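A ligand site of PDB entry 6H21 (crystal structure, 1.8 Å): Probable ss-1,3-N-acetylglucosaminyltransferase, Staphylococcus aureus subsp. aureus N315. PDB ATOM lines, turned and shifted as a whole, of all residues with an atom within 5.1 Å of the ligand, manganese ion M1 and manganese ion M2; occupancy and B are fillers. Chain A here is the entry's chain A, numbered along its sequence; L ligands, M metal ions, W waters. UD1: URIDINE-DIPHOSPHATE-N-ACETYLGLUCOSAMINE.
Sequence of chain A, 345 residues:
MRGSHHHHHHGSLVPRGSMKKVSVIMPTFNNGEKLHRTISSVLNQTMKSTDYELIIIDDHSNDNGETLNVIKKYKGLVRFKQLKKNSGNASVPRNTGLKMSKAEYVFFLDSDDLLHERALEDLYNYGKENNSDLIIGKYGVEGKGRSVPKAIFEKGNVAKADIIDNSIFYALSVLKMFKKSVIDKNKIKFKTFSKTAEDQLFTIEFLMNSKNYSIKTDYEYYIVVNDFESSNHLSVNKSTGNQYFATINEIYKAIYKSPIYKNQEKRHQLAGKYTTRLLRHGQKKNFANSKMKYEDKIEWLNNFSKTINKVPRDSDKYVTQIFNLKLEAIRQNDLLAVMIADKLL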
ATOM      1  N   PRO A  27      21.102  22.904 -14.538  1.00  0.00           N
ATOM      2  CA  PRO A  27      20.267  21.736 -14.255  1.00  0.00           C
ATOM      3  C   PRO A  27      20.017  20.897 -15.516  1.00  0.00           C
ATOM      4  O   PRO A  27      19.860  21.442 -16.602  1.00  0.00           O
ATOM      5  CB  PRO A  27      18.955  22.344 -13.731  1.00  0.00           C
ATOM      6  CG  PRO A  27      19.315  23.746 -13.303  1.00  0.00           C
ATOM      7  CD  PRO A  27      20.384  24.164 -14.288  1.00  0.00           C
ATOM      8  N   THR A  28      20.014  19.563 -15.354  1.00  0.00           N
ATOM      9  CA  THR A  28      19.758  18.614 -16.443  1.00  0.00           C
ATOM     10  C   THR A  28      18.638  17.659 -16.022  1.00  0.00           C
ATOM     11  O   THR A  28      18.449  17.424 -14.827  1.00  0.00           O
ATOM     12  CB  THR A  28      21.027  17.838 -16.828  1.00  0.00           C
ATOM     13  OG1 THR A  28      21.578  17.238 -15.655  1.00  0.00           O
ATOM     14  CG2 THR A  28      22.068  18.724 -17.482  1.00  0.00           C
ATOM     15  N   PHE A  29      17.922  17.116 -17.007  1.00  0.00           N
ATOM     16  CA  PHE A  29      16.907  16.098 -16.807  1.00  0.00           C
ATOM     17  C   PHE A  29      16.471  15.508 -18.148  1.00  0.00           C
ATOM     18  O   PHE A  29      15.768  16.169 -18.912  1.00  0.00           O
ATOM     19  CB  PHE A  29      15.692  16.664 -16.068  1.00  0.00           C
ATOM     20  CG  PHE A  29      14.644  15.626 -15.761  1.00  0.00           C
ATOM     21  CD1 PHE A  29      14.856  14.678 -14.781  1.00  0.00           C
ATOM     22  CD2 PHE A  29      13.450  15.596 -16.474  1.00  0.00           C
ATOM     23  CE1 PHE A  29      13.895  13.721 -14.499  1.00  0.00           C
ATOM     24  CE2 PHE A  29      12.489  14.639 -16.191  1.00  0.00           C
ATOM     25  CZ  PHE A  29      12.700  13.708 -15.198  1.00  0.00           C
ATOM     26  N   ASN A  31      17.956  14.791 -20.896  1.00  0.00           N
ATOM     27  CA  ASN A  31      18.384  15.599 -22.049  1.00  0.00           C
ATOM     28  C   ASN A  31      18.831  14.687 -23.198  1.00  0.00           C
ATOM     29  O   ASN A  31      18.434  14.883 -24.354  1.00  0.00           O
ATOM     30  CB  ASN A  31      19.483  16.586 -21.650  1.00  0.00           C
ATOM     31  CG  ASN A  31      18.978  17.644 -20.684  1.00  0.00           C
ATOM     32  OD1 ASN A  31      19.246  17.582 -19.489  1.00  0.00           O
ATOM     33  ND2 ASN A  31      18.212  18.587 -21.197  1.00  0.00           N
ATOM     34  N   ASP A  59      18.776  16.457 -12.073  1.00  0.00           N
ATOM     35  CA  ASP A  59      17.574  16.300 -11.243  1.00  0.00           C
ATOM     36  C   ASP A  59      17.065  14.846 -11.328  1.00  0.00           C
ATOM     37  O   ASP A  59      15.890  14.603 -11.623  1.00  0.00           O
ATOM     38  CB  ASP A  59      16.500  17.315 -11.639  1.00  0.00           C
ATOM     39  CG  ASP A  59      15.494  17.573 -10.530  1.00  0.00           C
ATOM     40  OD1 ASP A  59      15.666  16.994  -9.423  1.00  0.00           O
ATOM     41  OD2 ASP A  59      14.527  18.347 -10.775  1.00  0.00           O
ATOM     42  N   ASN A  86      13.882  13.271  -8.425  1.00  0.00           N
ATOM     43  CA  ASN A  86      13.409  14.287  -9.355  1.00  0.00           C
ATOM     44  C   ASN A  86      12.572  15.325  -8.585  1.00  0.00           C
ATOM     45  O   ASN A  86      11.528  15.001  -8.025  1.00  0.00           O
ATOM     46  CB  ASN A  86      12.624  13.674 -10.513  1.00  0.00           C
ATOM     47  CG  ASN A  86      12.204  14.700 -11.554  1.00  0.00           C
ATOM     48  OD1 ASN A  86      11.055  14.731 -11.979  1.00  0.00           O
ATOM     49  ND2 ASN A  86      13.133  15.548 -11.957  1.00  0.00           N
ATOM     50  N   SER A  87      13.050  16.567  -8.553  1.00  0.00           N
ATOM     51  CA  SER A  87      12.366  17.688  -7.865  1.00  0.00           C
ATOM     52  C   SER A  87      11.196  18.191  -8.710  1.00  0.00           C
ATOM     53  O   SER A  87      10.244  18.710  -8.157  1.00  0.00           O
ATOM     54  CB  SER A  87      13.328  18.801  -7.505  1.00  0.00           C
ATOM     55  OG  SER A  87      13.574  19.674  -8.592  1.00  0.00           O
ATOM     56  N   GLY A  88      11.280  18.049 -10.035  1.00  0.00           N
ATOM     57  CA  GLY A  88      10.175  18.386 -10.949  1.00  0.00           C
ATOM     58  C   GLY A  88      10.441  19.630 -11.793  1.00  0.00           C
ATOM     59  O   GLY A  88       9.765  19.833 -12.814  1.00  0.00           O
ATOM     60  N   ASN A  89      11.378  20.477 -11.364  1.00  0.00           N
ATOM     61  CA  ASN A  89      11.716  21.709 -12.083  1.00  0.00           C
ATOM     62  C   ASN A  89      13.112  22.164 -11.649  1.00  0.00           C
ATOM     63  O   ASN A  89      13.786  21.460 -10.903  1.00  0.00           O
ATOM     64  CB  ASN A  89      10.625  22.776 -11.899  1.00  0.00           C
ATOM     65  CG  ASN A  89      10.500  23.277 -10.475  1.00  0.00           C
ATOM     66  OD1 ASN A  89      11.469  23.362  -9.734  1.00  0.00           O
ATOM     67  ND2 ASN A  89       9.296  23.668 -10.090  1.00  0.00           N
ATOM     68  N   ALA A  90      13.516  23.358 -12.092  1.00  0.00           N
ATOM     69  CA  ALA A  90      14.913  23.783 -11.964  1.00  0.00           C
ATOM     70  C   ALA A  90      15.234  24.341 -10.572  1.00  0.00           C
ATOM     71  O   ALA A  90      16.400  24.539 -10.255  1.00  0.00           O
ATOM     72  CB  ALA A  90      15.218  24.801 -13.036  1.00  0.00           C
ATOM     73  N   PRO A  93      17.608  22.106  -7.940  1.00  0.00           N
ATOM     74  CA  PRO A  93      18.912  21.986  -8.600  1.00  0.00           C
ATOM     75  C   PRO A  93      19.691  23.310  -8.667  1.00  0.00           C
ATOM     76  O   PRO A  93      20.894  23.308  -8.523  1.00  0.00           O
ATOM     77  CB  PRO A  93      18.607  21.509 -10.033  1.00  0.00           C
ATOM     78  CG  PRO A  93      17.181  20.971  -9.990  1.00  0.00           C
ATOM     79  CD  PRO A  93      16.517  21.548  -8.752  1.00  0.00           C
ATOM     80  N   ARG A  94      18.986  24.434  -8.896  1.00  0.00           N
ATOM     81  CA  ARG A  94      19.623  25.746  -8.974  1.00  0.00           C
ATOM     82  C   ARG A  94      20.025  26.213  -7.573  1.00  0.00           C
ATOM     83  O   ARG A  94      21.048  26.866  -7.415  1.00  0.00           O
ATOM     84  CB  ARG A  94      18.694  26.778  -9.637  1.00  0.00           C
ATOM     85  CG  ARG A  94      18.568  26.637 -11.144  1.00  0.00           C
ATOM     86  CD  ARG A  94      17.560  27.632 -11.677  1.00  0.00           C
ATOM     87  NE  ARG A  94      17.464  27.670 -13.124  1.00  0.00           N
ATOM     88  CZ  ARG A  94      16.404  28.152 -13.773  1.00  0.00           C
ATOM     89  NH1 ARG A  94      15.376  28.610 -13.088  1.00  0.00           N
ATOM     90  NH2 ARG A  94      16.393  28.184 -15.095  1.00  0.00           N
ATOM     91  N   LEU A 109      22.192  28.580 -16.819  1.00  0.00           N
ATOM     92  CA  LEU A 109      22.069  28.068 -18.172  1.00  0.00           C
ATOM     93  C   LEU A 109      21.103  26.873 -18.190  1.00  0.00           C
ATOM     94  O   LEU A 109      21.337  25.884 -17.519  1.00  0.00           O
ATOM     95  CB  LEU A 109      23.457  27.670 -18.678  1.00  0.00           C
ATOM     96  CG  LEU A 109      23.473  26.907 -20.006  1.00  0.00           C
ATOM     97  CD1 LEU A 109      22.845  27.733 -21.120  1.00  0.00           C
ATOM     98  CD2 LEU A 109      24.892  26.489 -20.368  1.00  0.00           C
ATOM     99  N   ASP A 110      19.993  26.979 -18.936  1.00  0.00           N
ATOM    100  CA  ASP A 110      19.123  25.826 -19.187  1.00  0.00           C
ATOM    101  C   ASP A 110      19.816  24.851 -20.148  1.00  0.00           C
ATOM    102  O   ASP A 110      20.472  25.241 -21.111  1.00  0.00           O
ATOM    103  CB  ASP A 110      17.747  26.265 -19.693  1.00  0.00           C
ATOM    104  CG  ASP A 110      16.925  26.986 -18.634  1.00  0.00           C
ATOM    105  OD1 ASP A 110      17.332  26.943 -17.444  1.00  0.00           O
ATOM    106  OD2 ASP A 110      15.905  27.624 -19.024  1.00  0.00           O
ATOM    107  N   SER A 111      19.604  23.559 -19.890  1.00  0.00           N
ATOM    108  CA  SER A 111      20.337  22.457 -20.486  1.00  0.00           C
ATOM    109  C   SER A 111      19.981  22.209 -21.960  1.00  0.00           C
ATOM    110  O   SER A 111      20.546  21.306 -22.570  1.00  0.00           O
ATOM    111  CB  SER A 111      20.079  21.209 -19.696  1.00  0.00           C
ATOM    112  OG  SER A 111      18.692  20.871 -19.753  1.00  0.00           O
ATOM    113  N   ASP A 112      19.020  22.961 -22.514  1.00  0.00           N
ATOM    114  CA  ASP A 112      18.693  22.841 -23.936  1.00  0.00           C
ATOM    115  C   ASP A 112      19.196  24.065 -24.720  1.00  0.00           C
ATOM    116  O   ASP A 112      19.077  24.087 -25.933  1.00  0.00           O
ATOM    117  CB  ASP A 112      17.188  22.628 -24.176  1.00  0.00           C
ATOM    118  CG  ASP A 112      16.291  23.651 -23.525  1.00  0.00           C
ATOM    119  OD1 ASP A 112      16.804  24.488 -22.750  1.00  0.00           O
ATOM    120  OD2 ASP A 112      15.085  23.599 -23.767  1.00  0.00           O
ATOM    121  N   ASP A 113      19.788  25.046 -24.018  1.00  0.00           N
ATOM    122  CA  ASP A 113      20.179  26.326 -24.602  1.00  0.00           C
ATOM    123  C   ASP A 113      21.681  26.328 -24.918  1.00  0.00           C
ATOM    124  O   ASP A 113      22.387  25.342 -24.671  1.00  0.00           O
ATOM    125  CB  ASP A 113      19.745  27.480 -23.695  1.00  0.00           C
ATOM    126  CG  ASP A 113      18.227  27.651 -23.591  1.00  0.00           C
ATOM    127  OD1 ASP A 113      17.521  27.341 -24.573  1.00  0.00           O
ATOM    128  OD2 ASP A 113      17.769  28.083 -22.522  1.00  0.00           O
ATOM    129  N   SER A 173      13.512  36.355 -16.670  1.00  0.00           N
ATOM    130  CA  SER A 173      14.191  35.037 -16.584  1.00  0.00           C
ATOM    131  C   SER A 173      15.473  35.191 -15.770  1.00  0.00           C
ATOM    132  O   SER A 173      16.012  36.307 -15.670  1.00  0.00           O
ATOM    133  CB  SER A 173      14.508  34.444 -17.942  1.00  0.00           C
ATOM    134  OG  SER A 173      15.725  34.971 -18.483  1.00  0.00           O
ATOM    135  N   LEU A 175      18.180  33.785 -16.709  1.00  0.00           N
ATOM    136  CA  LEU A 175      19.218  33.415 -17.717  1.00  0.00           C
ATOM    137  C   LEU A 175      20.115  34.635 -17.980  1.00  0.00           C
ATOM    138  O   LEU A 175      20.134  35.235 -19.083  1.00  0.00           O
ATOM    139  CB  LEU A 175      18.532  32.869 -18.971  1.00  0.00           C
ATOM    140  CG  LEU A 175      17.524  31.739 -18.698  1.00  0.00           C
ATOM    141  CD1 LEU A 175      16.827  31.285 -19.970  1.00  0.00           C
ATOM    142  CD2 LEU A 175      18.191  30.567 -18.002  1.00  0.00           C
ATOM    143  N   GLU A 198       8.373  31.241 -10.214  1.00  0.00           N
ATOM    144  CA  GLU A 198       9.428  31.228  -9.207  1.00  0.00           C
ATOM    145  C   GLU A 198      10.687  31.934  -9.755  1.00  0.00           C
ATOM    146  O   GLU A 198      11.488  32.476  -9.006  1.00  0.00           O
ATOM    147  CB  GLU A 198       9.707  29.794  -8.773  1.00  0.00           C
ATOM    148  CG  GLU A 198      10.385  28.945  -9.839  1.00  0.00           C
ATOM    149  CD  GLU A 198       9.503  28.010 -10.648  1.00  0.00           C
ATOM    150  OE1 GLU A 198       8.294  28.301 -10.787  1.00  0.00           O
ATOM    151  OE2 GLU A 198      10.039  26.978 -11.126  1.00  0.00           O
ATOM    152  N   ASP A 199      10.867  31.905 -11.075  1.00  0.00           N
ATOM    153  CA  ASP A 199      12.018  32.534 -11.719  1.00  0.00           C
ATOM    154  C   ASP A 199      11.841  34.060 -11.629  1.00  0.00           C
ATOM    155  O   ASP A 199      12.796  34.811 -11.294  1.00  0.00           O
ATOM    156  CB  ASP A 199      12.223  31.979 -13.132  1.00  0.00           C
ATOM    157  CG  ASP A 199      12.732  30.547 -13.124  1.00  0.00           C
ATOM    158  OD1 ASP A 199      12.908  30.015 -12.018  1.00  0.00           O
ATOM    159  OD2 ASP A 199      12.973  29.975 -14.221  1.00  0.00           O
ATOM    160  N   VAL A 225      16.827  27.697 -27.316  1.00  0.00           N
ATOM    161  CA  VAL A 225      16.418  26.682 -28.308  1.00  0.00           C
ATOM    162  C   VAL A 225      14.989  26.227 -27.977  1.00  0.00           C
ATOM    163  O   VAL A 225      14.701  25.846 -26.839  1.00  0.00           O
ATOM    164  CB  VAL A 225      17.410  25.518 -28.357  1.00  0.00           C
ATOM    165  CG1 VAL A 225      17.026  24.476 -29.410  1.00  0.00           C
ATOM    166  CG2 VAL A 225      18.833  25.992 -28.597  1.00  0.00           C
ATOM    167  N   ASP A 227      11.969  23.529 -28.843  1.00  0.00           N
ATOM    168  CA  ASP A 227      11.596  22.228 -29.432  1.00  0.00           C
ATOM    169  C   ASP A 227      10.329  22.433 -30.274  1.00  0.00           C
ATOM    170  O   ASP A 227       9.445  21.587 -30.301  1.00  0.00           O
ATOM    171  CB  ASP A 227      11.393  21.140 -28.359  1.00  0.00           C
HETATM  172  C1' UD1 L   1      11.201  27.791 -19.374  1.00  0.00           C
HETATM  173  C2' UD1 L   1      11.478  29.268 -19.603  1.00  0.00           C
HETATM  174  C3' UD1 L   1      12.897  29.586 -19.160  1.00  0.00           C
HETATM  175  C4' UD1 L   1      13.129  29.127 -17.724  1.00  0.00           C
HETATM  176  C5' UD1 L   1      12.742  27.668 -17.539  1.00  0.00           C
HETATM  177  C6' UD1 L   1      12.854  27.254 -16.071  1.00  0.00           C
HETATM  178  C7' UD1 L   1      10.287  30.368 -21.440  1.00  0.00           C
HETATM  179  C8' UD1 L   1      10.217  30.618 -22.915  1.00  0.00           C
HETATM  180  N2' UD1 L   1      11.293  29.606 -21.022  1.00  0.00           N
HETATM  181  O1' UD1 L   1      12.113  27.065 -20.193  1.00  0.00           O
HETATM  182  O3' UD1 L   1      13.112  30.989 -19.246  1.00  0.00           O
HETATM  183  O4' UD1 L   1      14.502  29.285 -17.343  1.00  0.00           O
HETATM  184  O5' UD1 L   1      11.412  27.443 -18.002  1.00  0.00           O
HETATM  185  O6' UD1 L   1      11.783  27.812 -15.310  1.00  0.00           O
HETATM  186  O7' UD1 L   1       9.450  30.839 -20.665  1.00  0.00           O
HETATM  187  N1  UD1 L   1      14.687  20.716 -15.231  1.00  0.00           N
HETATM  188  C2  UD1 L   1      14.903  20.231 -13.923  1.00  0.00           C
HETATM  189  N3  UD1 L   1      14.090  19.312 -13.378  1.00  0.00           N
HETATM  190  C4  UD1 L   1      13.061  18.814 -14.071  1.00  0.00           C
HETATM  191  C5  UD1 L   1      12.814  19.266 -15.379  1.00  0.00           C
HETATM  192  C6  UD1 L   1      13.655  20.224 -15.940  1.00  0.00           C
HETATM  193  O2  UD1 L   1      15.859  20.665 -13.234  1.00  0.00           O
HETATM  194  O4  UD1 L   1      12.329  17.954 -13.551  1.00  0.00           O
HETATM  195  C1B UD1 L   1      15.609  21.717 -15.799  1.00  0.00           C
HETATM  196  C2B UD1 L   1      15.927  21.506 -17.281  1.00  0.00           C
HETATM  197  O2' UD1 L   1      16.882  20.461 -17.528  1.00  0.00           O
HETATM  198  C3B UD1 L   1      16.422  22.883 -17.677  1.00  0.00           C
HETATM  199  C4B UD1 L   1      15.585  23.824 -16.831  1.00  0.00           C
HETATM  200  O4B UD1 L   1      15.098  23.056 -15.723  1.00  0.00           O
HETATM  201  O3B UD1 L   1      17.801  23.074 -17.347  1.00  0.00           O
HETATM  202  C5B UD1 L   1      14.439  24.434 -17.624  1.00  0.00           C
HETATM  203  O5B UD1 L   1      13.871  23.454 -18.483  1.00  0.00           O
HETATM  204  PA  UD1 L   1      13.617  23.781 -20.025  1.00  0.00           P
HETATM  205  O1A UD1 L   1      13.190  22.519 -20.739  1.00  0.00           O
HETATM  206  O2A UD1 L   1      14.714  24.688 -20.576  1.00  0.00           O
HETATM  207  O3A UD1 L   1      12.313  24.707 -19.763  1.00  0.00           O
HETATM  208  PB  UD1 L   1      11.723  25.690 -20.884  1.00  0.00           P
HETATM  209  O1B UD1 L   1      10.214  25.554 -20.901  1.00  0.00           O
HETATM  210  O2B UD1 L   1      12.468  25.615 -22.191  1.00  0.00           O
HETATM  211 MN    MN M   1      14.668  25.380 -22.709  1.00  0.00          MN
HETATM  212 MN    MN M   2      13.530  22.498 -24.856  1.00  0.00          MN
HETATM  213  O   HOH W   1      15.094  26.462 -24.713  1.00  0.00           O
HETATM  214  O   HOH W   2      15.879  18.965 -19.214  1.00  0.00           O
HETATM  215  O   HOH W   3      12.527  21.998 -22.924  1.00  0.00           O
HETATM  216  O   HOH W   4      13.006  28.908 -23.098  1.00  0.00           O
HETATM  217  O   HOH W   5      13.735  31.254 -22.144  1.00  0.00           O
HETATM  218  O   HOH W   6      13.118  20.045 -19.275  1.00  0.00           O
HETATM  219  O   HOH W   7      15.259  26.865 -21.355  1.00  0.00           O
HETATM  220  O   HOH W   8      12.138  24.391 -24.796  1.00  0.00           O
HETATM  221  O   HOH W   9      14.164  31.552 -15.965  1.00  0.00           O
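OD2 of Asp 199 lies within hydrogen-bond range of O6' of the ligand.
O3B of the ligand is in hydrogen-bond range of O of Pro 27 (2.7 Å).
O4' of the ligand sits at hydrogen-bond distance from OD2 of Asp 110 (2.7 Å).
The side-chain carboxylate of Asp 59 lies within hydrogen-bond range of a nitrogen (N3) of the ligand, at 2.8 Å.
An oxygen (O3B) of the ligand sits at hydrogen-bond distance from the backbone NH (N) of Ser 111 (3.2 Å).
An oxygen (O2') of the ligand is in hydrogen-bond range of the side-chain hydroxyl (OG) of Ser 111, 2.9 Å away.
The side-chain amide nitrogen of Asn 86 sits at hydrogen-bond distance from an oxygen (O4) of the ligand, 3.0 Å away.
NH2 of Arg 94 is in hydrogen-bond range of O4' of the ligand (3.1 Å).
O4 of the ligand sits at hydrogen-bond distance from N of Asn 89 (3.5 Å).
The backbone carbonyl oxygen (O) of Asn 89 is in hydrogen-bond range of a nitrogen (N3) of the ligand (3.3 Å).
The side-chain carboxylate (OD2) of Asp 199 is in salt-bridge range of the guanidinium group (NH1) of Arg 94 (3.0 Å).
The side-chain hydroxyl (OG) of Ser 111 lies close to the backbone carbonyl oxygen (O) of Pro 27.
OD2 of Asp 59 sits at hydrogen-bond distance from N of Gly 88.
The backbone carbonyl oxygen (O) of Thr 28 sits at hydrogen-bond distance from the backbone NH (N) of Asp 59, 2.9 Å away.
ND2 of Asn 31 lies within hydrogen-bond range of OG of Ser 111 (2.7 Å).
OD1 of Asn 31 lies within hydrogen-bond range of N of Phe 29 (2.9 Å).
N of Leu 175 sits close to OG of Ser 173 (3.3 Å).
The side-chain carboxylate of Asp 113 is in hydrogen-bond range of the backbone NH of Val 225, 2.9 Å away.
O of Gly 88 lies close to O4 of the ligand (3.3 Å).
Merely in contact with the ligand: Thr 28 (3.6 Å), Phe 29 (3.5 Å), Ala 90 (3.2 Å), Pro 93 (3.5 Å), Ser 173 (3.9 Å) and Leu 175 (3.8 Å).
Hydrophobic or aromatic side chains that line the ligand: Pro 27, Phe 29, Ala 90, Pro 93 and Leu 175.
Of the 23 residues printed, 16 come within 4 Å of the ligand.
Residues that only touch manganese ion M1: Asp 113 (3.9 Å).
Two residues have an atom within 4 Å of manganese ion M1: Asp 112 and Asp 113.
Of the 23 residues printed, 1 comes within 4 Å of manganese ion M2.
Manganese ion M1 is bound by water W7, the side-chain carboxylate (OD2) of Asp 112, an oxygen (O2A) of the ligand, an oxygen (O2B) of the ligand, the side-chain carboxylate (OD1) of Asp 112 and water W1.
Manganese ion M2 is bound by the side-chain carboxylate (OD2) of Asp 112 (2.2 Å), water W3 (2.2 Å) and water W8 (2.4 Å).
Water W1 bridges the side-chain carboxylate (OD1) of Asp 113 and the backbone NH (N) of Val 225.
Water W2 lies within hydrogen-bond range of an oxygen (O2') of the ligand (2.5 Å), the backbone carbonyl oxygen of Phe 29 (2.8 Å), the side-chain amide nitrogen of Asn 31 (3.1 Å) and the side-chain hydroxyl of Ser 111 (3.4 Å).
Water W9 lies within hydrogen-bond range of OD2 of Asp 199 (2.6 Å) and O4' of the ligand (2.7 Å).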
